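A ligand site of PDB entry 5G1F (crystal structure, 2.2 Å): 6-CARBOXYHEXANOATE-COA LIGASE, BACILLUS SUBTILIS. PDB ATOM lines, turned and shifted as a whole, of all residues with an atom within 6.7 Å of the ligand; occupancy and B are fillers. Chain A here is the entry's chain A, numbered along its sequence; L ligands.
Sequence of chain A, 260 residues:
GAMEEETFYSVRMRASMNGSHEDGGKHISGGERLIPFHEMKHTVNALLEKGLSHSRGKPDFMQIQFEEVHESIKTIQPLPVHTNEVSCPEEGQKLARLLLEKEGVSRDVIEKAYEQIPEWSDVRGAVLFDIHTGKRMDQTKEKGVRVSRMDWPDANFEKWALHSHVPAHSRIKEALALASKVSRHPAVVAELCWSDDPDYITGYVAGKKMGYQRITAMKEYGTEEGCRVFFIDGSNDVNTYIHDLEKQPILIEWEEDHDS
An oxygen (O2) of the ligand sits at hydrogen-bond distance from the side-chain hydroxyl (OH) of Tyr 200 (2.5 Å). An oxygen (O4) of the ligand is in hydrogen-bond range of the side-chain hydroxyl (OG) of Ser 195. An oxygen (O1) of the ligand sits at hydrogen-bond distance from the side-chain hydroxyl (OH) of Tyr 212 (2.7 Å). NH2 of Arg 171 is in salt-bridge range of O3 of the ligand (2.8 Å). The guanidinium group (NH2) of Arg 214 is in salt-bridge range of an oxygen (O2) of the ligand (2.9 Å).
The guanidinium group of Arg 171 sits at hydrogen-bond distance from the side-chain hydroxyl of Ser 195 (3.3 Å). The side-chain hydroxyl (OG) of Ser 195 lies within hydrogen-bond range of the backbone NH (N) of Asp 197 (3.0 Å). The guanidinium group (NH1) of Arg 171 lies within salt-bridge range of the side-chain carboxylate (OD2) of Asp 197, at 3.5 Å. The backbone NH (N) of Tyr 204 sits at hydrogen-bond distance from the backbone carbonyl oxygen (O) of Cys 193. OH of Tyr 204 sits at hydrogen-bond distance from NH2 of Arg 228 (2.9 Å).
Merely in contact with the ligand: Ile 172, Thr 202, Ala 175 and Tyr 204. Nine residues have an atom within 4 Å of the ligand: Arg 171, Ile 172, Ala 175, Ser 195, Tyr 200, Thr 202, Tyr 204, Tyr 212 and Arg 214.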
ATOM      1  N   HIS A  54     -31.347  15.746  31.177  1.00  0.00           N
ATOM      2  CA  HIS A  54     -29.934  16.076  31.082  1.00  0.00           C
ATOM      3  C   HIS A  54     -29.744  17.447  31.758  1.00  0.00           C
ATOM      4  O   HIS A  54     -30.685  18.255  31.785  1.00  0.00           O
ATOM      5  CB  HIS A  54     -29.507  16.121  29.606  1.00  0.00           C
ATOM      6  CG  HIS A  54     -28.027  15.982  29.402  1.00  0.00           C
ATOM      7  ND1 HIS A  54     -27.155  17.048  29.523  1.00  0.00           N
ATOM      8  CD2 HIS A  54     -27.261  14.909  29.093  1.00  0.00           C
ATOM      9  CE1 HIS A  54     -25.912  16.638  29.306  1.00  0.00           C
ATOM     10  NE2 HIS A  54     -25.947  15.340  29.041  1.00  0.00           N
ATOM     11  N   VAL A 166     -12.448   1.783  38.862  1.00  0.00           N
ATOM     12  CA  VAL A 166     -12.980   3.007  38.205  1.00  0.00           C
ATOM     13  C   VAL A 166     -14.501   3.019  38.301  1.00  0.00           C
ATOM     14  O   VAL A 166     -15.131   1.990  38.147  1.00  0.00           O
ATOM     15  CB  VAL A 166     -12.605   3.045  36.705  1.00  0.00           C
ATOM     16  CG1 VAL A 166     -13.205   4.277  36.031  1.00  0.00           C
ATOM     17  CG2 VAL A 166     -11.095   3.042  36.529  1.00  0.00           C
ATOM     18  N   ARG A 171     -21.366   6.876  31.513  1.00  0.00           N
ATOM     19  CA  ARG A 171     -20.742   7.848  30.618  1.00  0.00           C
ATOM     20  C   ARG A 171     -19.262   7.534  30.411  1.00  0.00           C
ATOM     21  O   ARG A 171     -18.699   7.821  29.361  1.00  0.00           O
ATOM     22  CB  ARG A 171     -20.923   9.261  31.140  1.00  0.00           C
ATOM     23  CG  ARG A 171     -19.875   9.698  32.143  1.00  0.00           C
ATOM     24  CD  ARG A 171     -20.222  11.027  32.793  1.00  0.00           C
ATOM     25  NE  ARG A 171     -20.279  12.085  31.801  1.00  0.00           N
ATOM     26  CZ  ARG A 171     -21.029  13.172  31.898  1.00  0.00           C
ATOM     27  NH1 ARG A 171     -21.785  13.360  32.976  1.00  0.00           N
ATOM     28  NH2 ARG A 171     -21.043  14.063  30.915  1.00  0.00           N
ATOM     29  N   ILE A 172     -18.639   6.883  31.397  1.00  0.00           N
ATOM     30  CA  ILE A 172     -17.307   6.336  31.194  1.00  0.00           C
ATOM     31  C   ILE A 172     -17.373   5.133  30.266  1.00  0.00           C
ATOM     32  O   ILE A 172     -16.495   4.935  29.428  1.00  0.00           O
ATOM     33  CB  ILE A 172     -16.643   5.929  32.529  1.00  0.00           C
ATOM     34  CG1 ILE A 172     -16.296   7.182  33.332  1.00  0.00           C
ATOM     35  CG2 ILE A 172     -15.384   5.110  32.291  1.00  0.00           C
ATOM     36  CD1 ILE A 172     -16.127   6.944  34.819  1.00  0.00           C
ATOM     37  N   LYS A 173     -18.384   4.301  30.425  1.00  0.00           N
ATOM     38  CA  LYS A 173     -18.518   3.151  29.552  1.00  0.00           C
ATOM     39  C   LYS A 173     -18.669   3.607  28.099  1.00  0.00           C
ATOM     40  O   LYS A 173     -18.047   3.077  27.179  1.00  0.00           O
ATOM     41  CB  LYS A 173     -19.727   2.328  29.945  1.00  0.00           C
ATOM     42  CG  LYS A 173     -19.992   1.198  28.961  1.00  0.00           C
ATOM     43  CD  LYS A 173     -21.246   0.458  29.341  1.00  0.00           C
ATOM     44  CE  LYS A 173     -22.464   1.267  29.023  1.00  0.00           C
ATOM     45  NZ  LYS A 173     -23.647   0.374  29.099  1.00  0.00           N
ATOM     46  N   GLU A 174     -19.564   4.546  27.902  1.00  0.00           N
ATOM     47  CA  GLU A 174     -19.790   5.096  26.571  1.00  0.00           C
ATOM     48  C   GLU A 174     -18.523   5.719  25.997  1.00  0.00           C
ATOM     49  O   GLU A 174     -18.179   5.455  24.861  1.00  0.00           O
ATOM     50  CB  GLU A 174     -20.967   6.086  26.573  1.00  0.00           C
ATOM     51  CG  GLU A 174     -22.324   5.417  26.654  1.00  0.00           C
ATOM     52  CD  GLU A 174     -23.319   6.243  27.459  1.00  0.00           C
ATOM     53  OE1 GLU A 174     -23.155   7.474  27.491  1.00  0.00           O
ATOM     54  OE2 GLU A 174     -24.270   5.680  28.039  1.00  0.00           O
ATOM     55  N   ALA A 175     -17.758   6.455  26.794  1.00  0.00           N
ATOM     56  CA  ALA A 175     -16.647   7.215  26.259  1.00  0.00           C
ATOM     57  C   ALA A 175     -15.498   6.295  25.917  1.00  0.00           C
ATOM     58  O   ALA A 175     -14.839   6.459  24.897  1.00  0.00           O
ATOM     59  CB  ALA A 175     -16.199   8.285  27.241  1.00  0.00           C
ATOM     60  N   LEU A 176     -15.293   5.297  26.774  1.00  0.00           N
ATOM     61  CA  LEU A 176     -14.236   4.327  26.562  1.00  0.00           C
ATOM     62  C   LEU A 176     -14.552   3.376  25.394  1.00  0.00           C
ATOM     63  O   LEU A 176     -13.651   3.033  24.611  1.00  0.00           O
ATOM     64  CB  LEU A 176     -13.934   3.564  27.867  1.00  0.00           C
ATOM     65  CG  LEU A 176     -12.807   2.543  27.827  1.00  0.00           C
ATOM     66  CD1 LEU A 176     -11.556   3.052  27.134  1.00  0.00           C
ATOM     67  CD2 LEU A 176     -12.440   2.110  29.239  1.00  0.00           C
ATOM     68  N   CYS A 193     -10.529  14.867  24.186  1.00  0.00           N
ATOM     69  CA  CYS A 193     -11.938  14.926  24.511  1.00  0.00           C
ATOM     70  C   CYS A 193     -12.161  15.492  25.896  1.00  0.00           C
ATOM     71  O   CYS A 193     -11.555  15.048  26.849  1.00  0.00           O
ATOM     72  CB  CYS A 193     -12.577  13.530  24.428  1.00  0.00           C
ATOM     73  SG  CYS A 193     -14.353  13.533  24.816  1.00  0.00           S
ATOM     74  N   TRP A 194     -13.097  16.415  26.012  1.00  0.00           N
ATOM     75  CA  TRP A 194     -13.717  16.651  27.282  1.00  0.00           C
ATOM     76  C   TRP A 194     -15.163  17.041  27.072  1.00  0.00           C
ATOM     77  O   TRP A 194     -15.595  17.318  25.940  1.00  0.00           O
ATOM     78  CB  TRP A 194     -12.920  17.682  28.106  1.00  0.00           C
ATOM     79  CG  TRP A 194     -12.872  19.075  27.536  1.00  0.00           C
ATOM     80  CD1 TRP A 194     -13.712  20.113  27.844  1.00  0.00           C
ATOM     81  CD2 TRP A 194     -11.873  19.603  26.675  1.00  0.00           C
ATOM     82  NE1 TRP A 194     -13.337  21.245  27.159  1.00  0.00           N
ATOM     83  CE2 TRP A 194     -12.203  20.967  26.430  1.00  0.00           C
ATOM     84  CE3 TRP A 194     -10.748  19.069  26.055  1.00  0.00           C
ATOM     85  CZ2 TRP A 194     -11.423  21.792  25.613  1.00  0.00           C
ATOM     86  CZ3 TRP A 194      -9.984  19.890  25.222  1.00  0.00           C
ATOM     87  CH2 TRP A 194     -10.342  21.230  25.005  1.00  0.00           C
ATOM     88  N   SER A 195     -15.920  17.034  28.171  1.00  0.00           N
ATOM     89  CA  SER A 195     -17.362  17.048  28.130  1.00  0.00           C
ATOM     90  C   SER A 195     -17.927  18.446  27.888  1.00  0.00           C
ATOM     91  O   SER A 195     -17.294  19.451  28.235  1.00  0.00           O
ATOM     92  CB  SER A 195     -17.918  16.547  29.446  1.00  0.00           C
ATOM     93  OG  SER A 195     -19.316  16.424  29.337  1.00  0.00           O
ATOM     94  N   ASP A 196     -19.125  18.490  27.309  1.00  0.00           N
ATOM     95  CA  ASP A 196     -19.839  19.745  27.134  1.00  0.00           C
ATOM     96  C   ASP A 196     -20.822  19.955  28.278  1.00  0.00           C
ATOM     97  O   ASP A 196     -21.429  21.032  28.414  1.00  0.00           O
ATOM     98  CB  ASP A 196     -20.569  19.793  25.769  1.00  0.00           C
ATOM     99  CG  ASP A 196     -21.519  18.607  25.543  1.00  0.00           C
ATOM    100  OD1 ASP A 196     -21.455  17.592  26.264  1.00  0.00           O
ATOM    101  OD2 ASP A 196     -22.311  18.695  24.584  1.00  0.00           O
ATOM    102  N   ASP A 197     -20.954  18.943  29.128  1.00  0.00           N
ATOM    103  CA  ASP A 197     -21.733  19.028  30.361  1.00  0.00           C
ATOM    104  C   ASP A 197     -21.079  19.966  31.374  1.00  0.00           C
ATOM    105  O   ASP A 197     -19.940  19.735  31.794  1.00  0.00           O
ATOM    106  CB  ASP A 197     -21.878  17.610  30.930  1.00  0.00           C
ATOM    107  CG  ASP A 197     -22.760  17.536  32.163  1.00  0.00           C
ATOM    108  OD1 ASP A 197     -22.871  18.500  32.952  1.00  0.00           O
ATOM    109  OD2 ASP A 197     -23.291  16.441  32.412  1.00  0.00           O
ATOM    110  N   TYR A 200     -19.416  18.152  34.632  1.00  0.00           N
ATOM    111  CA  TYR A 200     -18.471  17.062  34.534  1.00  0.00           C
ATOM    112  C   TYR A 200     -17.198  17.598  33.884  1.00  0.00           C
ATOM    113  O   TYR A 200     -17.226  18.037  32.740  1.00  0.00           O
ATOM    114  CB  TYR A 200     -19.074  15.945  33.704  1.00  0.00           C
ATOM    115  CG  TYR A 200     -18.379  14.629  33.875  1.00  0.00           C
ATOM    116  CD1 TYR A 200     -18.594  13.831  35.012  1.00  0.00           C
ATOM    117  CD2 TYR A 200     -17.464  14.187  32.936  1.00  0.00           C
ATOM    118  CE1 TYR A 200     -17.918  12.628  35.182  1.00  0.00           C
ATOM    119  CE2 TYR A 200     -16.798  12.993  33.088  1.00  0.00           C
ATOM    120  CZ  TYR A 200     -17.026  12.212  34.202  1.00  0.00           C
ATOM    121  OH  TYR A 200     -16.321  11.051  34.302  1.00  0.00           O
ATOM    122  N   THR A 202     -13.938  16.051  33.991  1.00  0.00           N
ATOM    123  CA  THR A 202     -12.968  15.047  33.604  1.00  0.00           C
ATOM    124  C   THR A 202     -13.060  14.854  32.098  1.00  0.00           C
ATOM    125  O   THR A 202     -14.142  14.911  31.530  1.00  0.00           O
ATOM    126  CB  THR A 202     -13.225  13.692  34.301  1.00  0.00           C
ATOM    127  OG1 THR A 202     -13.074  13.815  35.720  1.00  0.00           O
ATOM    128  CG2 THR A 202     -12.230  12.643  33.804  1.00  0.00           C
ATOM    129  N   GLY A 203     -11.888  14.717  31.464  1.00  0.00           N
ATOM    130  CA  GLY A 203     -11.766  14.397  30.058  1.00  0.00           C
ATOM    131  C   GLY A 203     -10.669  13.379  29.822  1.00  0.00           C
ATOM    132  O   GLY A 203     -10.257  12.690  30.733  1.00  0.00           O
ATOM    133  N   TYR A 204     -10.233  13.238  28.598  1.00  0.00           N
ATOM    134  CA  TYR A 204      -9.172  12.282  28.320  1.00  0.00           C
ATOM    135  C   TYR A 204      -8.448  12.629  27.052  1.00  0.00           C
ATOM    136  O   TYR A 204      -8.983  13.316  26.195  1.00  0.00           O
ATOM    137  CB  TYR A 204      -9.714  10.846  28.208  1.00  0.00           C
ATOM    138  CG  TYR A 204     -10.718  10.629  27.090  1.00  0.00           C
ATOM    139  CD1 TYR A 204     -12.073  10.845  27.298  1.00  0.00           C
ATOM    140  CD2 TYR A 204     -10.321  10.134  25.880  1.00  0.00           C
ATOM    141  CE1 TYR A 204     -12.995  10.649  26.292  1.00  0.00           C
ATOM    142  CE2 TYR A 204     -11.230   9.931  24.862  1.00  0.00           C
ATOM    143  CZ  TYR A 204     -12.560  10.139  25.086  1.00  0.00           C
ATOM    144  OH  TYR A 204     -13.428   9.861  24.058  1.00  0.00           O
ATOM    145  N   TYR A 212      -6.174   4.908  27.159  1.00  0.00           N
ATOM    146  CA  TYR A 212      -7.147   5.891  27.554  1.00  0.00           C
ATOM    147  C   TYR A 212      -6.656   6.629  28.810  1.00  0.00           C
ATOM    148  O   TYR A 212      -6.630   6.069  29.887  1.00  0.00           O
ATOM    149  CB  TYR A 212      -8.445   5.142  27.857  1.00  0.00           C
ATOM    150  CG  TYR A 212      -9.641   5.986  28.169  1.00  0.00           C
ATOM    151  CD1 TYR A 212     -10.393   6.567  27.154  1.00  0.00           C
ATOM    152  CD2 TYR A 212     -10.138   6.058  29.457  1.00  0.00           C
ATOM    153  CE1 TYR A 212     -11.546   7.290  27.419  1.00  0.00           C
ATOM    154  CE2 TYR A 212     -11.287   6.766  29.734  1.00  0.00           C
ATOM    155  CZ  TYR A 212     -11.986   7.364  28.707  1.00  0.00           C
ATOM    156  OH  TYR A 212     -13.160   7.987  29.017  1.00  0.00           O
ATOM    157  N   ARG A 214      -7.230   9.357  31.424  1.00  0.00           N
ATOM    158  CA  ARG A 214      -8.209  10.243  32.008  1.00  0.00           C
ATOM    159  C   ARG A 214      -7.489  11.365  32.727  1.00  0.00           C
ATOM    160  O   ARG A 214      -6.433  11.167  33.292  1.00  0.00           O
ATOM    161  CB  ARG A 214      -9.123   9.481  32.944  1.00  0.00           C
ATOM    162  CG  ARG A 214      -9.804   8.318  32.259  1.00  0.00           C
ATOM    163  CD  ARG A 214     -10.536   7.467  33.271  1.00  0.00           C
ATOM    164  NE  ARG A 214     -11.699   8.164  33.795  1.00  0.00           N
ATOM    165  CZ  ARG A 214     -11.871   8.479  35.067  1.00  0.00           C
ATOM    166  NH1 ARG A 214     -10.919   8.248  35.946  1.00  0.00           N
ATOM    167  NH2 ARG A 214     -12.984   9.070  35.431  1.00  0.00           N
ATOM    168  N   ILE A 215      -8.026  12.575  32.584  1.00  0.00           N
ATOM    169  CA  ILE A 215      -7.426  13.763  33.165  1.00  0.00           C
ATOM    170  C   ILE A 215      -8.528  14.445  33.957  1.00  0.00           C
ATOM    171  O   ILE A 215      -9.523  14.878  33.385  1.00  0.00           O
ATOM    172  CB  ILE A 215      -6.891  14.697  32.060  1.00  0.00           C
ATOM    173  CG1 ILE A 215      -5.816  13.983  31.238  1.00  0.00           C
ATOM    174  CG2 ILE A 215      -6.306  15.974  32.641  1.00  0.00           C
ATOM    175  CD1 ILE A 215      -5.346  14.754  30.020  1.00  0.00           C
ATOM    176  N   ARG A 228     -14.304  17.231  21.125  1.00  0.00           N
ATOM    177  CA  ARG A 228     -13.880  15.911  20.671  1.00  0.00           C
ATOM    178  C   ARG A 228     -13.209  15.956  19.310  1.00  0.00           C
ATOM    179  O   ARG A 228     -13.835  16.311  18.301  1.00  0.00           O
ATOM    180  CB  ARG A 228     -15.048  14.930  20.618  1.00  0.00           C
ATOM    181  CG  ARG A 228     -14.630  13.568  20.098  1.00  0.00           C
ATOM    182  CD  ARG A 228     -15.668  12.492  20.355  1.00  0.00           C
ATOM    183  NE  ARG A 228     -15.449  11.817  21.633  1.00  0.00           N
ATOM    184  CZ  ARG A 228     -16.414  11.536  22.512  1.00  0.00           C
ATOM    185  NH1 ARG A 228     -17.672  11.888  22.246  1.00  0.00           N
ATOM    186  NH2 ARG A 228     -16.134  10.921  23.650  1.00  0.00           N
HETATM  187  C1  LIG L   1     -14.307   9.658  31.876  1.00  0.00           C
HETATM  188  O1  LIG L   1     -13.324   9.033  31.463  1.00  0.00           O
HETATM  189  O2  LIG L   1     -14.450   9.933  33.090  1.00  0.00           O
HETATM  190  C2  LIG L   1     -15.358  10.101  30.885  1.00  0.00           C
HETATM  191  C3  LIG L   1     -14.962  11.407  30.195  1.00  0.00           C
HETATM  192  C4  LIG L   1     -15.733  11.614  28.892  1.00  0.00           C
HETATM  193  C5  LIG L   1     -16.691  12.794  28.944  1.00  0.00           C
HETATM  194  C6  LIG L   1     -17.680  12.756  27.781  1.00  0.00           C
HETATM  195  C7  LIG L   1     -19.059  13.198  28.241  1.00  0.00           C
HETATM  196  O3  LIG L   1     -19.737  12.458  29.001  1.00  0.00           O
HETATM  197  O4  LIG L   1     -19.493  14.291  27.813  1.00  0.00           O
